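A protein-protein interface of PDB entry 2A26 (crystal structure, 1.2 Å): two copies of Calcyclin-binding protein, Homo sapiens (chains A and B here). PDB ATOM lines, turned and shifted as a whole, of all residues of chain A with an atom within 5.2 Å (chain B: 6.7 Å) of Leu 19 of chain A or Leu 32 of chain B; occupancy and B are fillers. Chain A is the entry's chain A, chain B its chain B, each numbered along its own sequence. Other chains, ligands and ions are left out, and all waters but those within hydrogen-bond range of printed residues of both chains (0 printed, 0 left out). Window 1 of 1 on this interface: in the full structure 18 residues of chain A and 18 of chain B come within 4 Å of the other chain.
Val 16 of chain A touches Val 28 of chain B, and with the chains exchanged Val 28 of chain A touches Val 16 of chain B.
Leu 19 of chain A touches Val 28 of chain B, and with the chains exchanged Val 28 of chain A touches Leu 19 of chain B.
Leu 19 of chain A touches Leu 32 of chain B, but with the chains exchanged Leu 32 of chain A does not touch Leu 19 of chain B (4.03 Å).
Lys 22 of chain A touches Leu 19 of chain B, but with the chains exchanged Leu 19 of chain A does not touch Lys 22 of chain B (4.01 Å).
10 positions are printed for both chains.
Of the 12 pairs that touch across the chains among the printed residues, 9 have their exchanged pair printed and touching as well.
Among the printed residues, pairs that only touch across the chains: Lys 22 of chain A with Lys 22 of chain B (3.4 Å), Glu 15 of chain A with Val 28 of chain B (3.4 Å), Val 16 of chain A with Val 28 of chain B (3.5 Å), Leu 19 of chain A with Val 28 of chain B (3.5 Å), Val 28 of chain A with Glu 15 of chain B (3.6 Å), Val 28 of chain A with Leu 19 of chain B (3.6 Å), Val 28 of chain A with Val 16 of chain B (3.7 Å), Glu 15 of chain A with Ala 23 of chain B (3.7 Å), Ala 23 of chain A with Glu 15 of chain B (3.7 Å), Leu 19 of chain A with Leu 32 of chain B (3.8 Å) and Lys 22 of chain A with Leu 19 of chain B (3.95 Å).
N of Thr 24 of chain B is in hydrogen-bond range of OE2 of Glu 15 of chain A (2.8 Å).
Of the 11 printed residues of chain A, 6 touch a printed residue of chain B.
Of the 21 printed residues of chain B, 8 touch a printed residue of chain A.
Hydrophobic or aromatic side chains of chain B within 4 Å of the printed part of chain A: Val 16, Leu 19, Ala 23, Val 28 and Leu 32.
Among the printed residues, no Asp or Glu carboxylate lies within 4 Å of a Lys or Arg side-chain nitrogen of the other chain.
Printed residues of chain B within 4 Å of Leu 19 of chain A: Val 28 (3.5 Å) and Leu 32 (3.8 Å).
Printed residues of chain B within 4 Å of Val 16 of chain A: Val 28.
Printed residues of chain A within 4 Å of Glu 15 of chain B: Ala 23 (3.7 Å) and Val 28 (3.6 Å).
Ala 31 of chain B touches none of the printed residues of chain A.
Glu 21 of chain A touches none of the printed residues of chain B.
The nearest printed residue of chain B that does not touch Leu 19 of chain A is Lys 22 of chain B (4.01 Å).
The nearest printed residue of chain A that does not touch Lys 22 of chain B is Leu 19 of chain A (4.01 Å).
The backbone carbonyl oxygen (O) of Ala 23 of chain B is in hydrogen-bond range of the guanidinium group (NH1) of Arg 29 of chain B (2.9 Å).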
ATOM      1  N   GLU A  15      18.725  17.311  -1.600  1.00  0.00           N
ATOM      2  CA  GLU A  15      19.516  18.372  -0.965  1.00  0.00           C
ATOM      3  C   GLU A  15      20.743  18.745  -1.783  1.00  0.00           C
ATOM      4  O   GLU A  15      21.045  19.935  -1.915  1.00  0.00           O
ATOM      5  CB  GLU A  15      19.899  17.998   0.461  1.00  0.00           C
ATOM      6  CG  GLU A  15      20.747  19.078   1.138  1.00  0.00           C
ATOM      7  CD  GLU A  15      20.817  18.894   2.624  1.00  0.00           C
ATOM      8  OE1 GLU A  15      21.784  18.293   3.098  1.00  0.00           O
ATOM      9  OE2 GLU A  15      19.887  19.390   3.354  1.00  0.00           O
ATOM     10  N   VAL A  16      21.501  17.764  -2.281  1.00  0.00           N
ATOM     11  CA  VAL A  16      22.671  18.090  -3.091  1.00  0.00           C
ATOM     12  C   VAL A  16      22.211  18.989  -4.223  1.00  0.00           C
ATOM     13  O   VAL A  16      22.871  20.001  -4.489  1.00  0.00           O
ATOM     14  CB  VAL A  16      23.399  16.854  -3.688  1.00  0.00           C
ATOM     15  CG1 VAL A  16      24.455  17.248  -4.772  1.00  0.00           C
ATOM     16  CG2 VAL A  16      24.048  16.057  -2.555  1.00  0.00           C
ATOM     17  N   LYS A  17      21.078  18.659  -4.864  1.00  0.00           N
ATOM     18  CA  LYS A  17      20.491  19.492  -5.918  1.00  0.00           C
ATOM     19  C   LYS A  17      20.240  20.924  -5.398  1.00  0.00           C
ATOM     20  O   LYS A  17      20.589  21.907  -6.063  1.00  0.00           O
ATOM     21  CB  LYS A  17      19.187  18.885  -6.486  1.00  0.00           C
ATOM     22  CG  LYS A  17      19.300  17.746  -7.475  1.00  0.00           C
ATOM     23  CD  LYS A  17      17.985  16.926  -7.553  1.00  0.00           C
ATOM     24  CE  LYS A  17      16.824  17.721  -8.156  1.00  0.00           C
ATOM     25  NZ  LYS A  17      15.563  16.916  -8.316  1.00  0.00           N
ATOM     26  N   VAL A  18      19.603  21.057  -4.232  1.00  0.00           N
ATOM     27  CA  VAL A  18      19.362  22.374  -3.667  1.00  0.00           C
ATOM     28  C   VAL A  18      20.648  23.176  -3.452  1.00  0.00           C
ATOM     29  O   VAL A  18      20.704  24.374  -3.764  1.00  0.00           O
ATOM     30  CB  VAL A  18      18.511  22.296  -2.375  1.00  0.00           C
ATOM     31  CG1 VAL A  18      18.465  23.628  -1.670  1.00  0.00           C
ATOM     32  CG2 VAL A  18      17.078  21.862  -2.700  1.00  0.00           C
ATOM     33  N   LEU A  19      21.682  22.525  -2.923  1.00  0.00           N
ATOM     34  CA  LEU A  19      22.958  23.211  -2.719  1.00  0.00           C
ATOM     35  C   LEU A  19      23.595  23.625  -4.025  1.00  0.00           C
ATOM     36  O   LEU A  19      24.215  24.696  -4.091  1.00  0.00           O
ATOM     37  CB  LEU A  19      23.903  22.345  -1.904  1.00  0.00           C
ATOM     38  CG  LEU A  19      23.417  22.064  -0.492  1.00  0.00           C
ATOM     39  CD1 LEU A  19      24.528  21.295   0.188  1.00  0.00           C
ATOM     40  CD2 LEU A  19      23.019  23.299   0.310  1.00  0.00           C
ATOM     41  N   LEU A  20      23.430  22.802  -5.057  1.00  0.00           N
ATOM     42  CA  LEU A  20      23.959  23.096  -6.384  1.00  0.00           C
ATOM     43  C   LEU A  20      23.236  24.272  -7.071  1.00  0.00           C
ATOM     44  O   LEU A  20      23.753  24.839  -8.033  1.00  0.00           O
ATOM     45  CB  LEU A  20      23.952  21.845  -7.266  1.00  0.00           C
ATOM     46  CG  LEU A  20      25.145  20.911  -7.060  1.00  0.00           C
ATOM     47  CD1 LEU A  20      24.827  19.580  -7.707  1.00  0.00           C
ATOM     48  CD2 LEU A  20      26.444  21.494  -7.588  1.00  0.00           C
ATOM     49  N   GLU A  21      22.035  24.613  -6.617  1.00  0.00           N
ATOM     50  CA  GLU A  21      21.343  25.833  -7.051  1.00  0.00           C
ATOM     51  C   GLU A  21      22.133  27.052  -6.618  1.00  0.00           C
ATOM     52  O   GLU A  21      22.071  28.061  -7.319  1.00  0.00           O
ATOM     53  CB  GLU A  21      19.922  25.910  -6.454  1.00  0.00           C
ATOM     54  CG  GLU A  21      18.995  24.828  -6.975  1.00  0.00           C
ATOM     55  CD  GLU A  21      17.660  24.775  -6.278  1.00  0.00           C
ATOM     56  OE1 GLU A  21      17.380  25.636  -5.414  1.00  0.00           O
ATOM     57  OE2 GLU A  21      16.887  23.836  -6.576  1.00  0.00           O
ATOM     58  N   LYS A  22      22.839  26.930  -5.480  1.00  0.00           N
ATOM     59  CA  LYS A  22      23.495  28.026  -4.736  1.00  0.00           C
ATOM     60  C   LYS A  22      25.004  28.181  -4.960  1.00  0.00           C
ATOM     61  O   LYS A  22      25.574  29.283  -5.034  1.00  0.00           O
ATOM     62  CB  LYS A  22      23.270  27.765  -3.251  1.00  0.00           C
ATOM     63  CG  LYS A  22      21.826  27.478  -3.078  1.00  0.00           C
ATOM     64  CD  LYS A  22      21.359  27.455  -1.670  1.00  0.00           C
ATOM     65  CE  LYS A  22      19.874  27.103  -1.523  1.00  0.00           C
ATOM     66  NZ  LYS A  22      18.826  28.104  -1.830  1.00  0.00           N
ATOM     67  N   ALA A  23      25.721  27.095  -5.071  1.00  0.00           N
ATOM     68  CA  ALA A  23      27.173  27.170  -5.034  1.00  0.00           C
ATOM     69  C   ALA A  23      27.748  27.951  -6.239  1.00  0.00           C
ATOM     70  O   ALA A  23      27.185  27.771  -7.341  1.00  0.00           O
ATOM     71  CB  ALA A  23      27.656  25.719  -4.986  1.00  0.00           C
ATOM     72  N   VAL A  28      33.944  23.768  -5.057  1.00  0.00           N
ATOM     73  CA  VAL A  28      32.763  23.331  -4.307  1.00  0.00           C
ATOM     74  C   VAL A  28      31.734  22.743  -5.237  1.00  0.00           C
ATOM     75  O   VAL A  28      31.165  21.697  -4.949  1.00  0.00           O
ATOM     76  CB  VAL A  28      32.218  24.494  -3.479  1.00  0.00           C
ATOM     77  CG1 VAL A  28      30.946  24.074  -2.720  1.00  0.00           C
ATOM     78  CG2 VAL A  28      33.283  24.989  -2.521  1.00  0.00           C
ATOM     79  N   LEU A  32      30.410  18.840  -5.131  1.00  0.00           N
ATOM     80  CA  LEU A  32      28.992  18.499  -5.035  1.00  0.00           C
ATOM     81  C   LEU A  32      28.516  17.736  -6.253  1.00  0.00           C
ATOM     82  O   LEU A  32      27.651  16.865  -6.091  1.00  0.00           O
ATOM     83  CB  LEU A  32      28.174  19.776  -4.822  1.00  0.00           C
ATOM     84  CG  LEU A  32      28.319  20.462  -3.465  1.00  0.00           C
ATOM     85  CD1 LEU A  32      27.635  21.825  -3.527  1.00  0.00           C
ATOM     86  CD2 LEU A  32      27.723  19.609  -2.343  1.00  0.00           C
ATOM     87  N   GLU B  15      32.263  29.924   1.172  1.00  0.00           N
ATOM     88  CA  GLU B  15      31.150  29.235   0.533  1.00  0.00           C
ATOM     89  C   GLU B  15      30.786  27.911   1.196  1.00  0.00           C
ATOM     90  O   GLU B  15      29.617  27.620   1.377  1.00  0.00           O
ATOM     91  CB  GLU B  15      31.394  28.999  -0.924  1.00  0.00           C
ATOM     92  CG  GLU B  15      30.252  28.249  -1.578  1.00  0.00           C
ATOM     93  CD  GLU B  15      30.141  28.495  -3.028  1.00  0.00           C
ATOM     94  OE1 GLU B  15      30.623  27.663  -3.803  1.00  0.00           O
ATOM     95  OE2 GLU B  15      29.598  29.593  -3.384  1.00  0.00           O
ATOM     96  N   VAL B  16      31.802  27.118   1.576  1.00  0.00           N
ATOM     97  CA  VAL B  16      31.475  25.876   2.241  1.00  0.00           C
ATOM     98  C   VAL B  16      30.733  26.129   3.564  1.00  0.00           C
ATOM     99  O   VAL B  16      29.798  25.396   3.898  1.00  0.00           O
ATOM    100  CB  VAL B  16      32.752  25.058   2.474  1.00  0.00           C
ATOM    101  CG1 VAL B  16      32.430  23.895   3.371  1.00  0.00           C
ATOM    102  CG2 VAL B  16      33.299  24.567   1.107  1.00  0.00           C
ATOM    103  N   VAL B  18      28.769  28.724   4.207  1.00  0.00           N
ATOM    104  CA  VAL B  18      27.404  29.143   3.813  1.00  0.00           C
ATOM    105  C   VAL B  18      26.567  27.908   3.526  1.00  0.00           C
ATOM    106  O   VAL B  18      25.390  27.804   3.961  1.00  0.00           O
ATOM    107  CB  VAL B  18      27.466  30.073   2.567  1.00  0.00           C
ATOM    108  CG1 VAL B  18      26.126  30.242   1.886  1.00  0.00           C
ATOM    109  CG2 VAL B  18      28.029  31.460   2.900  1.00  0.00           C
ATOM    110  N   LEU B  19      27.108  26.936   2.784  1.00  0.00           N
ATOM    111  CA  LEU B  19      26.337  25.739   2.439  1.00  0.00           C
ATOM    112  C   LEU B  19      26.127  24.829   3.638  1.00  0.00           C
ATOM    113  O   LEU B  19      25.062  24.226   3.763  1.00  0.00           O
ATOM    114  CB  LEU B  19      26.977  25.026   1.263  1.00  0.00           C
ATOM    115  CG  LEU B  19      27.135  25.834  -0.010  1.00  0.00           C
ATOM    116  CD1 LEU B  19      27.851  24.984  -1.040  1.00  0.00           C
ATOM    117  CD2 LEU B  19      25.774  26.354  -0.538  1.00  0.00           C
ATOM    118  N   LEU B  20      27.104  24.713   4.540  1.00  0.00           N
ATOM    119  CA  LEU B  20      26.910  23.942   5.756  1.00  0.00           C
ATOM    120  C   LEU B  20      25.793  24.525   6.617  1.00  0.00           C
ATOM    121  O   LEU B  20      25.082  23.766   7.299  1.00  0.00           O
ATOM    122  CB  LEU B  20      28.195  23.847   6.570  1.00  0.00           C
ATOM    123  CG  LEU B  20      29.150  22.762   6.047  1.00  0.00           C
ATOM    124  CD1 LEU B  20      30.548  22.969   6.562  1.00  0.00           C
ATOM    125  CD2 LEU B  20      28.631  21.393   6.449  1.00  0.00           C
ATOM    126  N   GLU B  21      25.599  25.837   6.627  1.00  0.00           N
ATOM    127  CA  GLU B  21      24.497  26.383   7.412  1.00  0.00           C
ATOM    128  C   GLU B  21      23.146  25.901   6.849  1.00  0.00           C
ATOM    129  O   GLU B  21      22.198  25.776   7.613  1.00  0.00           O
ATOM    130  CB  GLU B  21      24.555  27.897   7.378  1.00  0.00           C
ATOM    131  CG  GLU B  21      23.505  28.581   8.231  1.00  0.00           C
ATOM    132  CD  GLU B  21      23.646  30.101   8.277  1.00  0.00           C
ATOM    133  OE1 GLU B  21      23.931  30.714   7.213  1.00  0.00           O
ATOM    134  OE2 GLU B  21      23.422  30.703   9.323  1.00  0.00           O
ATOM    135  N   LYS B  22      23.052  25.645   5.550  1.00  0.00           N
ATOM    136  CA  LYS B  22      21.832  25.186   4.890  1.00  0.00           C
ATOM    137  C   LYS B  22      21.645  23.668   4.950  1.00  0.00           C
ATOM    138  O   LYS B  22      20.530  23.180   4.961  1.00  0.00           O
ATOM    139  CB  LYS B  22      21.868  25.579   3.401  1.00  0.00           C
ATOM    140  CG  LYS B  22      21.934  27.082   3.153  1.00  0.00           C
ATOM    141  CD  LYS B  22      22.174  27.368   1.664  1.00  0.00           C
ATOM    142  CE  LYS B  22      22.462  28.820   1.404  1.00  0.00           C
ATOM    143  NZ  LYS B  22      21.218  29.597   1.431  1.00  0.00           N
ATOM    144  N   ALA B  23      22.716  22.906   4.945  1.00  0.00           N
ATOM    145  CA  ALA B  23      22.651  21.458   4.724  1.00  0.00           C
ATOM    146  C   ALA B  23      22.148  20.768   5.969  1.00  0.00           C
ATOM    147  O   ALA B  23      22.670  21.003   7.072  1.00  0.00           O
ATOM    148  CB  ALA B  23      23.996  20.958   4.342  1.00  0.00           C
ATOM    149  N   THR B  24      21.240  19.808   5.790  1.00  0.00           N
ATOM    150  CA  THR B  24      20.716  19.013   6.907  1.00  0.00           C
ATOM    151  C   THR B  24      20.989  17.509   6.769  1.00  0.00           C
ATOM    152  O   THR B  24      20.895  16.837   7.797  1.00  0.00           O
ATOM    153  CB  THR B  24      19.159  19.262   7.062  1.00  0.00           C
ATOM    154  OG1 THR B  24      18.542  18.651   5.920  1.00  0.00           O
ATOM    155  CG2 THR B  24      18.804  20.743   6.949  1.00  0.00           C
ATOM    156  N   ARG B  27      24.813  12.780   4.844  1.00  0.00           N
ATOM    157  CA  ARG B  27      25.725  12.436   3.751  1.00  0.00           C
ATOM    158  C   ARG B  27      26.273  13.701   3.068  1.00  0.00           C
ATOM    159  O   ARG B  27      27.462  13.773   2.670  1.00  0.00           O
ATOM    160  CB  ARG B  27      24.989  11.560   2.740  1.00  0.00           C
ATOM    161  CG  ARG B  27      25.901  11.109   1.591  1.00  0.00           C
ATOM    162  CD  ARG B  27      25.310  10.088   0.684  1.00  0.00           C
ATOM    163  NE  ARG B  27      26.306   9.839  -0.352  1.00  0.00           N
ATOM    164  CZ  ARG B  27      26.546   8.652  -0.884  1.00  0.00           C
ATOM    165  NH1 ARG B  27      25.862   7.607  -0.451  1.00  0.00           N
ATOM    166  NH2 ARG B  27      27.440   8.550  -1.868  1.00  0.00           N
ATOM    167  N   VAL B  28      25.400  14.687   2.898  1.00  0.00           N
ATOM    168  CA  VAL B  28      25.805  15.937   2.254  1.00  0.00           C
ATOM    169  C   VAL B  28      26.700  16.763   3.172  1.00  0.00           C
ATOM    170  O   VAL B  28      27.711  17.325   2.724  1.00  0.00           O
ATOM    171  CB  VAL B  28      24.555  16.707   1.794  1.00  0.00           C
ATOM    172  CG1 VAL B  28      24.966  17.973   1.097  1.00  0.00           C
ATOM    173  CG2 VAL B  28      23.673  15.775   0.867  1.00  0.00           C
ATOM    174  N   ARG B  29      26.323  16.858   4.438  1.00  0.00           N
ATOM    175  CA  ARG B  29      27.185  17.535   5.401  1.00  0.00           C
ATOM    176  C   ARG B  29      28.573  16.913   5.477  1.00  0.00           C
ATOM    177  O   ARG B  29      29.574  17.635   5.522  1.00  0.00           O
ATOM    178  CB  ARG B  29      26.560  17.517   6.794  1.00  0.00           C
ATOM    179  CG  ARG B  29      25.282  18.348   6.915  1.00  0.00           C
ATOM    180  CD  ARG B  29      24.781  18.465   8.351  1.00  0.00           C
ATOM    181  NE  ARG B  29      25.748  19.179   9.175  1.00  0.00           N
ATOM    182  CZ  ARG B  29      25.994  20.476   9.133  1.00  0.00           C
ATOM    183  NH1 ARG B  29      25.225  21.250   8.392  1.00  0.00           N
ATOM    184  NH2 ARG B  29      26.973  20.958   9.873  1.00  0.00           N
ATOM    185  N   ASP B  30      28.665  15.590   5.439  1.00  0.00           N
ATOM    186  CA  ASP B  30      29.968  14.935   5.450  1.00  0.00           C
ATOM    187  C   ASP B  30      30.808  15.307   4.248  1.00  0.00           C
ATOM    188  O   ASP B  30      32.026  15.534   4.395  1.00  0.00           O
ATOM    189  CB  ASP B  30      29.818  13.424   5.553  1.00  0.00           C
ATOM    190  CG  ASP B  30      29.381  12.957   6.931  1.00  0.00           C
ATOM    191  OD1 ASP B  30      29.364  13.716   7.929  1.00  0.00           O
ATOM    192  OD2 ASP B  30      29.037  11.760   7.094  1.00  0.00           O
ATOM    193  N   ALA B  31      30.225  15.363   3.061  1.00  0.00           N
ATOM    194  CA  ALA B  31      30.952  15.780   1.864  1.00  0.00           C
ATOM    195  C   ALA B  31      31.446  17.210   1.977  1.00  0.00           C
ATOM    196  O   ALA B  31      32.569  17.540   1.607  1.00  0.00           O
ATOM    197  CB  ALA B  31      30.073  15.631   0.625  1.00  0.00           C
ATOM    198  N   LEU B  32      30.602  18.109   2.471  1.00  0.00           N
ATOM    199  CA  LEU B  32      30.996  19.500   2.668  1.00  0.00           C
ATOM    200  C   LEU B  32      32.073  19.622   3.735  1.00  0.00           C
ATOM    201  O   LEU B  32      33.007  20.425   3.578  1.00  0.00           O
ATOM    202  CB  LEU B  32      29.781  20.358   3.044  1.00  0.00           C
ATOM    203  CG  LEU B  32      28.779  20.596   1.933  1.00  0.00           C
ATOM    204  CD1 LEU B  32      27.492  21.143   2.542  1.00  0.00           C
ATOM    205  CD2 LEU B  32      29.363  21.597   0.923  1.00  0.00           C
ATOM    206  N   THR B  33      31.959  18.905   4.850  1.00  0.00           N
ATOM    207  CA  THR B  33      32.929  18.969   5.930  1.00  0.00           C
ATOM    208  C   THR B  33      34.290  18.452   5.448  1.00  0.00           C
ATOM    209  O   THR B  33      35.326  19.005   5.847  1.00  0.00           O
ATOM    210  CB  THR B  33      32.425  18.202   7.133  1.00  0.00           C
ATOM    211  OG1 THR B  33      31.253  18.875   7.606  1.00  0.00           O
ATOM    212  CG2 THR B  33      33.461  18.258   8.297  1.00  0.00           C
ATOM    213  N   ALA B  34      34.305  17.443   4.581  1.00  0.00           N
ATOM    214  CA  ALA B  34      35.578  16.949   4.018  1.00  0.00           C
ATOM    215  C   ALA B  34      36.259  18.033   3.201  1.00  0.00           C
ATOM    216  O   ALA B  34      37.482  18.237   3.311  1.00  0.00           O
ATOM    217  CB  ALA B  34      35.364  15.676   3.179  1.00  0.00           C
ATOM    218  N   GLU B  35      35.480  18.766   2.400  1.00  0.00           N
ATOM    219  CA  GLU B  35      36.061  19.851   1.640  1.00  0.00           C
ATOM    220  C   GLU B  35      36.533  20.983   2.533  1.00  0.00           C
ATOM    221  O   GLU B  35      37.627  21.543   2.329  1.00  0.00           O
ATOM    222  CB  GLU B  35      35.079  20.355   0.543  1.00  0.00           C
ATOM    223  CG  GLU B  35      35.850  21.026  -0.650  1.00  0.00           C
ATOM    224  CD  GLU B  35      36.784  20.171  -1.541  1.00  0.00           C
ATOM    225  OE1 GLU B  35      36.656  18.915  -1.678  1.00  0.00           O
ATOM    226  OE2 GLU B  35      37.755  20.742  -2.171  1.00  0.00           O
ATOM    227  N   LYS B  36      35.743  21.309   3.549  1.00  0.00           N
ATOM    228  CA  LYS B  36      36.112  22.342   4.520  1.00  0.00           C
ATOM    229  C   LYS B  36      37.466  22.038   5.165  1.00  0.00           C
ATOM    230  O   LYS B  36      38.295  22.910   5.269  1.00  0.00           O
ATOM    231  CB  LYS B  36      35.011  22.466   5.609  1.00  0.00           C
ATOM    232  CG  LYS B  36      35.285  23.580   6.591  1.00  0.00           C
ATOM    233  CD  LYS B  36      34.050  23.756   7.490  1.00  0.00           C
ATOM    234  CE  LYS B  36      34.162  24.825   8.531  1.00  0.00           C
ATOM    235  NZ  LYS B  36      34.900  24.296   9.734  1.00  0.00           N
ATOM    236  N   SER B  37      37.655  20.789   5.583  1.00  0.00           N
ATOM    237  CA  SER B  37      38.875  20.323   6.236  1.00  0.00           C
ATOM    238  C   SER B  37      40.095  20.501   5.338  1.00  0.00           C
ATOM    239  O   SER B  37      41.181  20.882   5.782  1.00  0.00           O
ATOM    240  CB  SER B  37      38.748  18.836   6.601  1.00  0.00           C
ATOM    241  OG  SER B  37      39.926  18.435   7.290  1.00  0.00           O
ATOM    242  N   ILE B  39      40.338  22.668   2.735  1.00  0.00           N
ATOM    243  CA  ILE B  39      40.588  24.067   2.514  1.00  0.00           C
ATOM    244  C   ILE B  39      41.251  24.682   3.735  1.00  0.00           C
ATOM    245  O   ILE B  39      42.193  25.488   3.609  1.00  0.00           O
ATOM    246  CB  ILE B  39      39.270  24.778   2.151  1.00  0.00           C
ATOM    247  CG1 ILE B  39      38.652  24.241   0.853  1.00  0.00           C
ATOM    248  CG2 ILE B  39      39.508  26.272   2.102  1.00  0.00           C
ATOM    249  CD1 ILE B  39      37.179  24.527   0.752  1.00  0.00           C
